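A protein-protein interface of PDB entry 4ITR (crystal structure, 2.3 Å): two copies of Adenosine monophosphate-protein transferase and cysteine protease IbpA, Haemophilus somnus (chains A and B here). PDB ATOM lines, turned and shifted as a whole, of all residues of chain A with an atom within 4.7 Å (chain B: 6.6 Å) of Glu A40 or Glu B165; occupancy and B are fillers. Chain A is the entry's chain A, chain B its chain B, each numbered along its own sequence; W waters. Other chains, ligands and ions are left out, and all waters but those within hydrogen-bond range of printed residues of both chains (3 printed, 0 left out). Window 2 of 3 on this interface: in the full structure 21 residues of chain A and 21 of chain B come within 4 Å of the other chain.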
ATOM      1  N   LYS A  38      10.459   6.055 -15.906  1.00  0.00           N
ATOM      2  CA  LYS A  38      11.009   6.043 -14.553  1.00  0.00           C
ATOM      3  C   LYS A  38       9.988   6.461 -13.500  1.00  0.00           C
ATOM      4  O   LYS A  38      10.318   6.570 -12.319  1.00  0.00           O
ATOM      5  CB  LYS A  38      12.247   6.937 -14.467  1.00  0.00           C
ATOM      6  CG  LYS A  38      13.487   6.340 -15.118  1.00  0.00           C
ATOM      7  CD  LYS A  38      14.628   7.345 -15.155  1.00  0.00           C
ATOM      8  CE  LYS A  38      15.888   6.728 -15.744  1.00  0.00           C
ATOM      9  NZ  LYS A  38      16.940   7.753 -15.998  1.00  0.00           N
ATOM     10  N   ASN A  39       8.752   6.699 -13.927  1.00  0.00           N
ATOM     11  CA  ASN A  39       7.678   6.998 -12.989  1.00  0.00           C
ATOM     12  C   ASN A  39       7.337   5.765 -12.161  1.00  0.00           C
ATOM     13  O   ASN A  39       7.022   4.708 -12.711  1.00  0.00           O
ATOM     14  CB  ASN A  39       6.438   7.507 -13.725  1.00  0.00           C
ATOM     15  CG  ASN A  39       5.324   7.909 -12.777  1.00  0.00           C
ATOM     16  OD1 ASN A  39       4.442   7.111 -12.463  1.00  0.00           O
ATOM     17  ND2 ASN A  39       5.365   9.150 -12.308  1.00  0.00           N
ATOM     18  N   GLU A  40       7.397   5.904 -10.840  1.00  0.00           N
ATOM     19  CA  GLU A  40       7.263   4.757  -9.944  1.00  0.00           C
ATOM     20  C   GLU A  40       5.890   4.086  -9.964  1.00  0.00           C
ATOM     21  O   GLU A  40       5.795   2.869  -9.787  1.00  0.00           O
ATOM     22  CB  GLU A  40       7.661   5.141  -8.516  1.00  0.00           C
ATOM     23  CG  GLU A  40       9.165   5.285  -8.321  1.00  0.00           C
ATOM     24  CD  GLU A  40       9.915   3.982  -8.544  1.00  0.00           C
ATOM     25  OE1 GLU A  40       9.307   2.900  -8.393  1.00  0.00           O
ATOM     26  OE2 GLU A  40      11.120   4.037  -8.870  1.00  0.00           O
ATOM     27  N   LYS A  41       4.833   4.868 -10.179  1.00  0.00           N
ATOM     28  CA  LYS A  41       3.489   4.302 -10.299  1.00  0.00           C
ATOM     29  C   LYS A  41       3.389   3.414 -11.529  1.00  0.00           C
ATOM     30  O   LYS A  41       2.795   2.338 -11.482  1.00  0.00           O
ATOM     31  CB  LYS A  41       2.427   5.397 -10.390  1.00  0.00           C
ATOM     32  CG  LYS A  41       2.223   6.195  -9.119  1.00  0.00           C
ATOM     33  CD  LYS A  41       1.134   7.236  -9.323  1.00  0.00           C
ATOM     34  CE  LYS A  41       1.546   8.583  -8.757  1.00  0.00           C
ATOM     35  NZ  LYS A  41       0.649   9.671  -9.231  1.00  0.00           N
ATOM     36  N   PHE A  42       3.961   3.884 -12.635  1.00  0.00           N
ATOM     37  CA  PHE A  42       4.021   3.095 -13.856  1.00  0.00           C
ATOM     38  C   PHE A  42       4.816   1.820 -13.614  1.00  0.00           C
ATOM     39  O   PHE A  42       4.417   0.737 -14.044  1.00  0.00           O
ATOM     40  CB  PHE A  42       4.664   3.899 -14.988  1.00  0.00           C
ATOM     41  CG  PHE A  42       4.949   3.084 -16.216  1.00  0.00           C
ATOM     42  CD1 PHE A  42       3.923   2.726 -17.078  1.00  0.00           C
ATOM     43  CD2 PHE A  42       6.239   2.659 -16.501  1.00  0.00           C
ATOM     44  CE1 PHE A  42       4.179   1.969 -18.204  1.00  0.00           C
ATOM     45  CE2 PHE A  42       6.502   1.901 -17.624  1.00  0.00           C
ATOM     46  CZ  PHE A  42       5.470   1.554 -18.475  1.00  0.00           C
ATOM     47  N   LEU A  43       5.943   1.955 -12.920  1.00  0.00           N
ATOM     48  CA  LEU A  43       6.802   0.815 -12.620  1.00  0.00           C
ATOM     49  C   LEU A  43       6.096  -0.195 -11.718  1.00  0.00           C
ATOM     50  O   LEU A  43       6.102  -1.396 -12.003  1.00  0.00           O
ATOM     51  CB  LEU A  43       8.113   1.283 -11.985  1.00  0.00           C
ATOM     52  CG  LEU A  43       9.057   2.072 -12.897  1.00  0.00           C
ATOM     53  CD1 LEU A  43      10.200   2.681 -12.104  1.00  0.00           C
ATOM     54  CD2 LEU A  43       9.596   1.194 -14.020  1.00  0.00           C
ATOM     55  N   ASP A  44       5.489   0.292 -10.637  1.00  0.00           N
ATOM     56  CA  ASP A  44       4.730  -0.567  -9.731  1.00  0.00           C
ATOM     57  C   ASP A  44       3.615  -1.301 -10.469  1.00  0.00           C
ATOM     58  O   ASP A  44       3.355  -2.474 -10.211  1.00  0.00           O
ATOM     59  CB  ASP A  44       4.142   0.243  -8.569  1.00  0.00           C
ATOM     60  CG  ASP A  44       5.106   0.388  -7.407  1.00  0.00           C
ATOM     61  OD1 ASP A  44       6.214  -0.185  -7.473  1.00  0.00           O
ATOM     62  OD2 ASP A  44       4.745   1.065  -6.419  1.00  0.00           O
ATOM     63  N   ARG A  47       5.365  -3.957 -12.388  1.00  0.00           N
ATOM     64  CA  ARG A  47       5.812  -4.965 -11.431  1.00  0.00           C
ATOM     65  C   ARG A  47       4.679  -5.902 -11.022  1.00  0.00           C
ATOM     66  O   ARG A  47       4.855  -7.121 -10.983  1.00  0.00           O
ATOM     67  CB  ARG A  47       6.403  -4.299 -10.184  1.00  0.00           C
ATOM     68  CG  ARG A  47       7.718  -3.567 -10.411  1.00  0.00           C
ATOM     69  CD  ARG A  47       8.200  -2.882  -9.139  1.00  0.00           C
ATOM     70  NE  ARG A  47       9.431  -2.127  -9.358  1.00  0.00           N
ATOM     71  CZ  ARG A  47       9.529  -0.803  -9.271  1.00  0.00           C
ATOM     72  NH1 ARG A  47       8.470  -0.069  -8.956  1.00  0.00           N
ATOM     73  NH2 ARG A  47      10.694  -0.212  -9.492  1.00  0.00           N
ATOM     74  N   THR B 160      10.159  17.166  -2.674  1.00  0.00           N
ATOM     75  CA  THR B 160       9.359  16.567  -3.740  1.00  0.00           C
ATOM     76  C   THR B 160       8.897  15.168  -3.353  1.00  0.00           C
ATOM     77  O   THR B 160       9.460  14.550  -2.449  1.00  0.00           O
ATOM     78  CB  THR B 160      10.132  16.481  -5.073  1.00  0.00           C
ATOM     79  OG1 THR B 160      11.217  15.554  -4.948  1.00  0.00           O
ATOM     80  CG2 THR B 160      10.670  17.846  -5.472  1.00  0.00           C
ATOM     81  N   VAL B 161       7.867  14.678  -4.039  1.00  0.00           N
ATOM     82  CA  VAL B 161       7.400  13.306  -3.866  1.00  0.00           C
ATOM     83  C   VAL B 161       8.516  12.321  -4.224  1.00  0.00           C
ATOM     84  O   VAL B 161       8.647  11.261  -3.609  1.00  0.00           O
ATOM     85  CB  VAL B 161       6.144  13.027  -4.728  1.00  0.00           C
ATOM     86  CG1 VAL B 161       5.702  11.579  -4.595  1.00  0.00           C
ATOM     87  CG2 VAL B 161       5.009  13.956  -4.332  1.00  0.00           C
ATOM     88  N   GLN B 162       9.332  12.693  -5.207  1.00  0.00           N
ATOM     89  CA  GLN B 162      10.431  11.850  -5.676  1.00  0.00           C
ATOM     90  C   GLN B 162      11.474  11.598  -4.588  1.00  0.00           C
ATOM     91  O   GLN B 162      11.963  10.475  -4.438  1.00  0.00           O
ATOM     92  CB  GLN B 162      11.102  12.487  -6.896  1.00  0.00           C
ATOM     93  CG  GLN B 162      11.081  11.629  -8.157  1.00  0.00           C
ATOM     94  CD  GLN B 162       9.804  11.788  -8.965  1.00  0.00           C
ATOM     95  OE1 GLN B 162       8.712  11.454  -8.501  1.00  0.00           O
ATOM     96  NE2 GLN B 162       9.937  12.301 -10.184  1.00  0.00           N
ATOM     97  N   MET B 163      11.819  12.644  -3.839  1.00  0.00           N
ATOM     98  CA  MET B 163      12.765  12.517  -2.729  1.00  0.00           C
ATOM     99  C   MET B 163      12.258  11.508  -1.699  1.00  0.00           C
ATOM    100  O   MET B 163      13.019  10.691  -1.179  1.00  0.00           O
ATOM    101  CB  MET B 163      12.981  13.872  -2.048  1.00  0.00           C
ATOM    102  CG  MET B 163      13.610  14.945  -2.930  1.00  0.00           C
ATOM    103  SD  MET B 163      13.655  16.557  -2.109  1.00  0.00           S
ATOM    104  CE  MET B 163      14.307  17.597  -3.420  1.00  0.00           C
ATOM    105  N   ILE B 164      10.961  11.579  -1.420  1.00  0.00           N
ATOM    106  CA  ILE B 164      10.321  10.717  -0.434  1.00  0.00           C
ATOM    107  C   ILE B 164      10.302   9.261  -0.900  1.00  0.00           C
ATOM    108  O   ILE B 164      10.526   8.344  -0.103  1.00  0.00           O
ATOM    109  CB  ILE B 164       8.893  11.211  -0.128  1.00  0.00           C
ATOM    110  CG1 ILE B 164       8.943  12.627   0.453  1.00  0.00           C
ATOM    111  CG2 ILE B 164       8.191  10.281   0.834  1.00  0.00           C
ATOM    112  CD1 ILE B 164       7.592  13.181   0.850  1.00  0.00           C
ATOM    113  N   GLU B 165      10.040   9.057  -2.191  1.00  0.00           N
ATOM    114  CA  GLU B 165      10.102   7.726  -2.790  1.00  0.00           C
ATOM    115  C   GLU B 165      11.505   7.141  -2.648  1.00  0.00           C
ATOM    116  O   GLU B 165      11.667   5.974  -2.290  1.00  0.00           O
ATOM    117  CB  GLU B 165       9.704   7.777  -4.271  1.00  0.00           C
ATOM    118  CG  GLU B 165       8.227   8.078  -4.527  1.00  0.00           C
ATOM    119  CD  GLU B 165       7.901   8.205  -6.003  1.00  0.00           C
ATOM    120  OE1 GLU B 165       8.842   8.349  -6.813  1.00  0.00           O
ATOM    121  OE2 GLU B 165       6.703   8.168  -6.356  1.00  0.00           O
ATOM    122  N   ASN B 166      12.514   7.958  -2.939  1.00  0.00           N
ATOM    123  CA  ASN B 166      13.905   7.547  -2.776  1.00  0.00           C
ATOM    124  C   ASN B 166      14.229   7.269  -1.311  1.00  0.00           C
ATOM    125  O   ASN B 166      14.943   6.317  -0.992  1.00  0.00           O
ATOM    126  CB  ASN B 166      14.854   8.619  -3.329  1.00  0.00           C
ATOM    127  CG  ASN B 166      14.760   8.765  -4.837  1.00  0.00           C
ATOM    128  OD1 ASN B 166      14.477   7.803  -5.550  1.00  0.00           O
ATOM    129  ND2 ASN B 166      15.001   9.975  -5.331  1.00  0.00           N
ATOM    130  N   LEU B 167      13.698   8.107  -0.424  1.00  0.00           N
ATOM    131  CA  LEU B 167      13.892   7.931   1.014  1.00  0.00           C
ATOM    132  C   LEU B 167      13.250   6.638   1.511  1.00  0.00           C
ATOM    133  O   LEU B 167      13.887   5.859   2.216  1.00  0.00           O
ATOM    134  CB  LEU B 167      13.336   9.129   1.791  1.00  0.00           C
ATOM    135  CG  LEU B 167      13.350   8.996   3.316  1.00  0.00           C
ATOM    136  CD1 LEU B 167      14.761   8.777   3.823  1.00  0.00           C
ATOM    137  CD2 LEU B 167      12.731  10.211   3.983  1.00  0.00           C
ATOM    138  N   ASN B 168      11.992   6.417   1.139  1.00  0.00           N
ATOM    139  CA  ASN B 168      11.272   5.211   1.543  1.00  0.00           C
ATOM    140  C   ASN B 168      11.989   3.933   1.113  1.00  0.00           C
ATOM    141  O   ASN B 168      12.096   2.984   1.887  1.00  0.00           O
ATOM    142  CB  ASN B 168       9.841   5.227   0.999  1.00  0.00           C
ATOM    143  CG  ASN B 168       9.066   3.970   1.357  1.00  0.00           C
ATOM    144  OD1 ASN B 168       8.874   3.085   0.523  1.00  0.00           O
ATOM    145  ND2 ASN B 168       8.627   3.881   2.607  1.00  0.00           N
ATOM    146  N   HIS B 169      12.479   3.920  -0.124  1.00  0.00           N
ATOM    147  CA  HIS B 169      13.202   2.766  -0.655  1.00  0.00           C
ATOM    148  C   HIS B 169      14.498   2.528   0.111  1.00  0.00           C
ATOM    149  O   HIS B 169      14.850   1.386   0.416  1.00  0.00           O
ATOM    150  CB  HIS B 169      13.503   2.963  -2.144  1.00  0.00           C
ATOM    151  CG  HIS B 169      14.237   1.819  -2.774  1.00  0.00           C
ATOM    152  ND1 HIS B 169      13.613   0.650  -3.157  1.00  0.00           N
ATOM    153  CD2 HIS B 169      15.544   1.669  -3.099  1.00  0.00           C
ATOM    154  CE1 HIS B 169      14.503  -0.170  -3.686  1.00  0.00           C
ATOM    155  NE2 HIS B 169      15.682   0.422  -3.661  1.00  0.00           N
ATOM    156  N   GLY B 170      15.208   3.610   0.419  1.00  0.00           N
ATOM    157  CA  GLY B 170      16.454   3.515   1.159  1.00  0.00           C
ATOM    158  C   GLY B 170      16.260   2.974   2.565  1.00  0.00           C
ATOM    159  O   GLY B 170      17.174   2.384   3.145  1.00  0.00           O
ATOM    160  N   ARG B 179      10.309  -5.424  -5.468  1.00  0.00           N
ATOM    161  CA  ARG B 179       9.177  -5.131  -4.597  1.00  0.00           C
ATOM    162  C   ARG B 179       8.419  -3.897  -5.079  1.00  0.00           C
ATOM    163  O   ARG B 179       9.000  -3.001  -5.693  1.00  0.00           O
ATOM    164  CB  ARG B 179       9.642  -4.915  -3.158  1.00  0.00           C
ATOM    165  CG  ARG B 179      10.598  -5.975  -2.631  1.00  0.00           C
ATOM    166  CD  ARG B 179      10.036  -7.386  -2.784  1.00  0.00           C
ATOM    167  NE  ARG B 179       8.671  -7.509  -2.274  1.00  0.00           N
ATOM    168  CZ  ARG B 179       8.360  -7.716  -0.997  1.00  0.00           C
ATOM    169  NH1 ARG B 179       9.318  -7.813  -0.085  1.00  0.00           N
ATOM    170  NH2 ARG B 179       7.090  -7.818  -0.629  1.00  0.00           N
ATOM    171  N   LEU B 181       6.860  -0.343  -4.629  1.00  0.00           N
ATOM    172  CA  LEU B 181       7.182   0.794  -3.775  1.00  0.00           C
ATOM    173  C   LEU B 181       5.954   1.193  -2.968  1.00  0.00           C
ATOM    174  O   LEU B 181       5.970   1.169  -1.734  1.00  0.00           O
ATOM    175  CB  LEU B 181       7.681   1.975  -4.609  1.00  0.00           C
ATOM    176  CG  LEU B 181       8.115   3.207  -3.814  1.00  0.00           C
ATOM    177  CD1 LEU B 181       9.260   2.862  -2.881  1.00  0.00           C
ATOM    178  CD2 LEU B 181       8.511   4.331  -4.746  1.00  0.00           C
ATOM    179  N   TYR B 182       4.890   1.553  -3.678  1.00  0.00           N
ATOM    180  CA  TYR B 182       3.616   1.878  -3.051  1.00  0.00           C
ATOM    181  C   TYR B 182       2.826   0.610  -2.756  1.00  0.00           C
ATOM    182  O   TYR B 182       3.033  -0.425  -3.396  1.00  0.00           O
ATOM    183  CB  TYR B 182       2.798   2.794  -3.964  1.00  0.00           C
ATOM    184  CG  TYR B 182       3.381   4.178  -4.125  1.00  0.00           C
ATOM    185  CD1 TYR B 182       3.096   5.180  -3.208  1.00  0.00           C
ATOM    186  CD2 TYR B 182       4.212   4.485  -5.196  1.00  0.00           C
ATOM    187  CE1 TYR B 182       3.623   6.445  -3.349  1.00  0.00           C
ATOM    188  CE2 TYR B 182       4.746   5.750  -5.344  1.00  0.00           C
ATOM    189  CZ  TYR B 182       4.447   6.723  -4.419  1.00  0.00           C
ATOM    190  OH  TYR B 182       4.974   7.984  -4.566  1.00  0.00           O
ATOM    191  N   LEU B 204      -0.307  12.486  -0.262  1.00  0.00           N
ATOM    192  CA  LEU B 204       1.138  12.576  -0.062  1.00  0.00           C
ATOM    193  C   LEU B 204       1.633  13.827  -0.780  1.00  0.00           C
ATOM    194  O   LEU B 204       2.421  14.599  -0.236  1.00  0.00           O
ATOM    195  CB  LEU B 204       1.857  11.336  -0.604  1.00  0.00           C
ATOM    196  CG  LEU B 204       3.389  11.395  -0.575  1.00  0.00           C
ATOM    197  CD1 LEU B 204       3.905  11.475   0.850  1.00  0.00           C
ATOM    198  CD2 LEU B 204       4.004  10.208  -1.297  1.00  0.00           C
ATOM    199  N   PHE B 238       3.117   3.930   1.191  1.00  0.00           N
ATOM    200  CA  PHE B 238       4.066   2.908   0.766  1.00  0.00           C
ATOM    201  C   PHE B 238       3.772   1.523   1.348  1.00  0.00           C
ATOM    202  O   PHE B 238       3.105   1.393   2.373  1.00  0.00           O
ATOM    203  CB  PHE B 238       5.495   3.366   1.078  1.00  0.00           C
ATOM    204  CG  PHE B 238       5.885   4.633   0.367  1.00  0.00           C
ATOM    205  CD1 PHE B 238       6.327   4.593  -0.947  1.00  0.00           C
ATOM    206  CD2 PHE B 238       5.797   5.866   1.003  1.00  0.00           C
ATOM    207  CE1 PHE B 238       6.679   5.753  -1.615  1.00  0.00           C
ATOM    208  CE2 PHE B 238       6.147   7.032   0.339  1.00  0.00           C
ATOM    209  CZ  PHE B 238       6.589   6.974  -0.971  1.00  0.00           C
ATOM    210  N   MET B 245       9.919   6.495   7.508  1.00  0.00           N
ATOM    211  CA  MET B 245       9.911   7.580   6.536  1.00  0.00           C
ATOM    212  C   MET B 245       9.323   8.865   7.117  1.00  0.00           C
ATOM    213  O   MET B 245       9.895   9.945   6.966  1.00  0.00           O
ATOM    214  CB  MET B 245       9.110   7.146   5.311  1.00  0.00           C
ATOM    215  CG  MET B 245       9.078   8.146   4.189  1.00  0.00           C
ATOM    216  SD  MET B 245       7.524   7.993   3.303  1.00  0.00           S
ATOM    217  CE  MET B 245       6.386   8.616   4.537  1.00  0.00           C
HETATM  218  O   HOH W   1       5.423   7.575  -8.801  1.00  0.00           O
HETATM  219  O   HOH W   2       8.261   8.844  -9.640  1.00  0.00           O
HETATM  220  O   HOH W   3       1.620  -0.366  -5.872  1.00  0.00           O
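Hydrophobic or aromatic side chains of chain B that line the printed part of chain A: Leu B181 and Tyr B182.
Among the printed residues, no Asp or Glu carboxylate lies within 4 Å of a Lys or Arg side-chain nitrogen of the other chain.
OE1 of Glu A40 is in salt-bridge range of NH1 of Arg A47 (3.1 Å).
The guanidinium group (NH1) of Arg A47 is in salt-bridge range of the side-chain carboxylate (OD1) of Asp A44, at 2.7 Å.
The side-chain carboxylate (OE2) of Glu B165 is in hydrogen-bond range of the side-chain hydroxyl (OH) of Tyr B182 (2.5 Å).
Glu A40 touches two residues of chain B.
Of chain A, only Glu A40 comes within 4 Å of Glu B165.
Of the printed residues of chain A, Tyr B182 touches Asp A44.
Of the printed residues of chain A, Arg B179 touches Arg A47 (3.5 Å).
Lys A41 touches none of the printed residues of chain B.
Gln B162 touches none of the printed residues of chain A.
The nearest residue of chain B that does not touch Glu A40 is Tyr B182 (4.4 Å).
The nearest printed residue of chain A that does not touch Glu B165 is Lys A41 (5.4 Å).
The nearest printed residue of chain A that does not touch Tyr B182 is Glu A40 (4.4 Å).
Water W1 lies within hydrogen-bond range of the side-chain carboxylate of Glu B165 (2.8 Å), the backbone NH of Lys A41 (3.1 Å) and the backbone NH of Glu A40 (3.3 Å).
Water W3 lies within hydrogen-bond range of the backbone carbonyl oxygen of Tyr B182 (2.9 Å) and the side-chain carboxylate of Asp A44 (3.5 Å).
Water W2 lies within hydrogen-bond range of OE1 of Gln B162 (2.9 Å), OE1 of Glu B165 (2.9 Å) and N of Glu A40 (3.3 Å).
No position is printed for both chains.
Of the 5 pairs that touch across the chains among the printed residues, none has its exchanged pair printed and touching as well.
Among the printed residues, merely in contact across the chains: Glu A40 with Glu B165, Arg A47 with Arg B179 and Glu A40 with Leu B181.
The side-chain carboxylate (OD1) of Asp A44 is in hydrogen-bond range of the backbone NH (N) of Leu B181, at 2.9 Å.
The side-chain carboxylate of Asp A44 lies within hydrogen-bond range of the backbone NH of Tyr B182 (2.8 Å).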
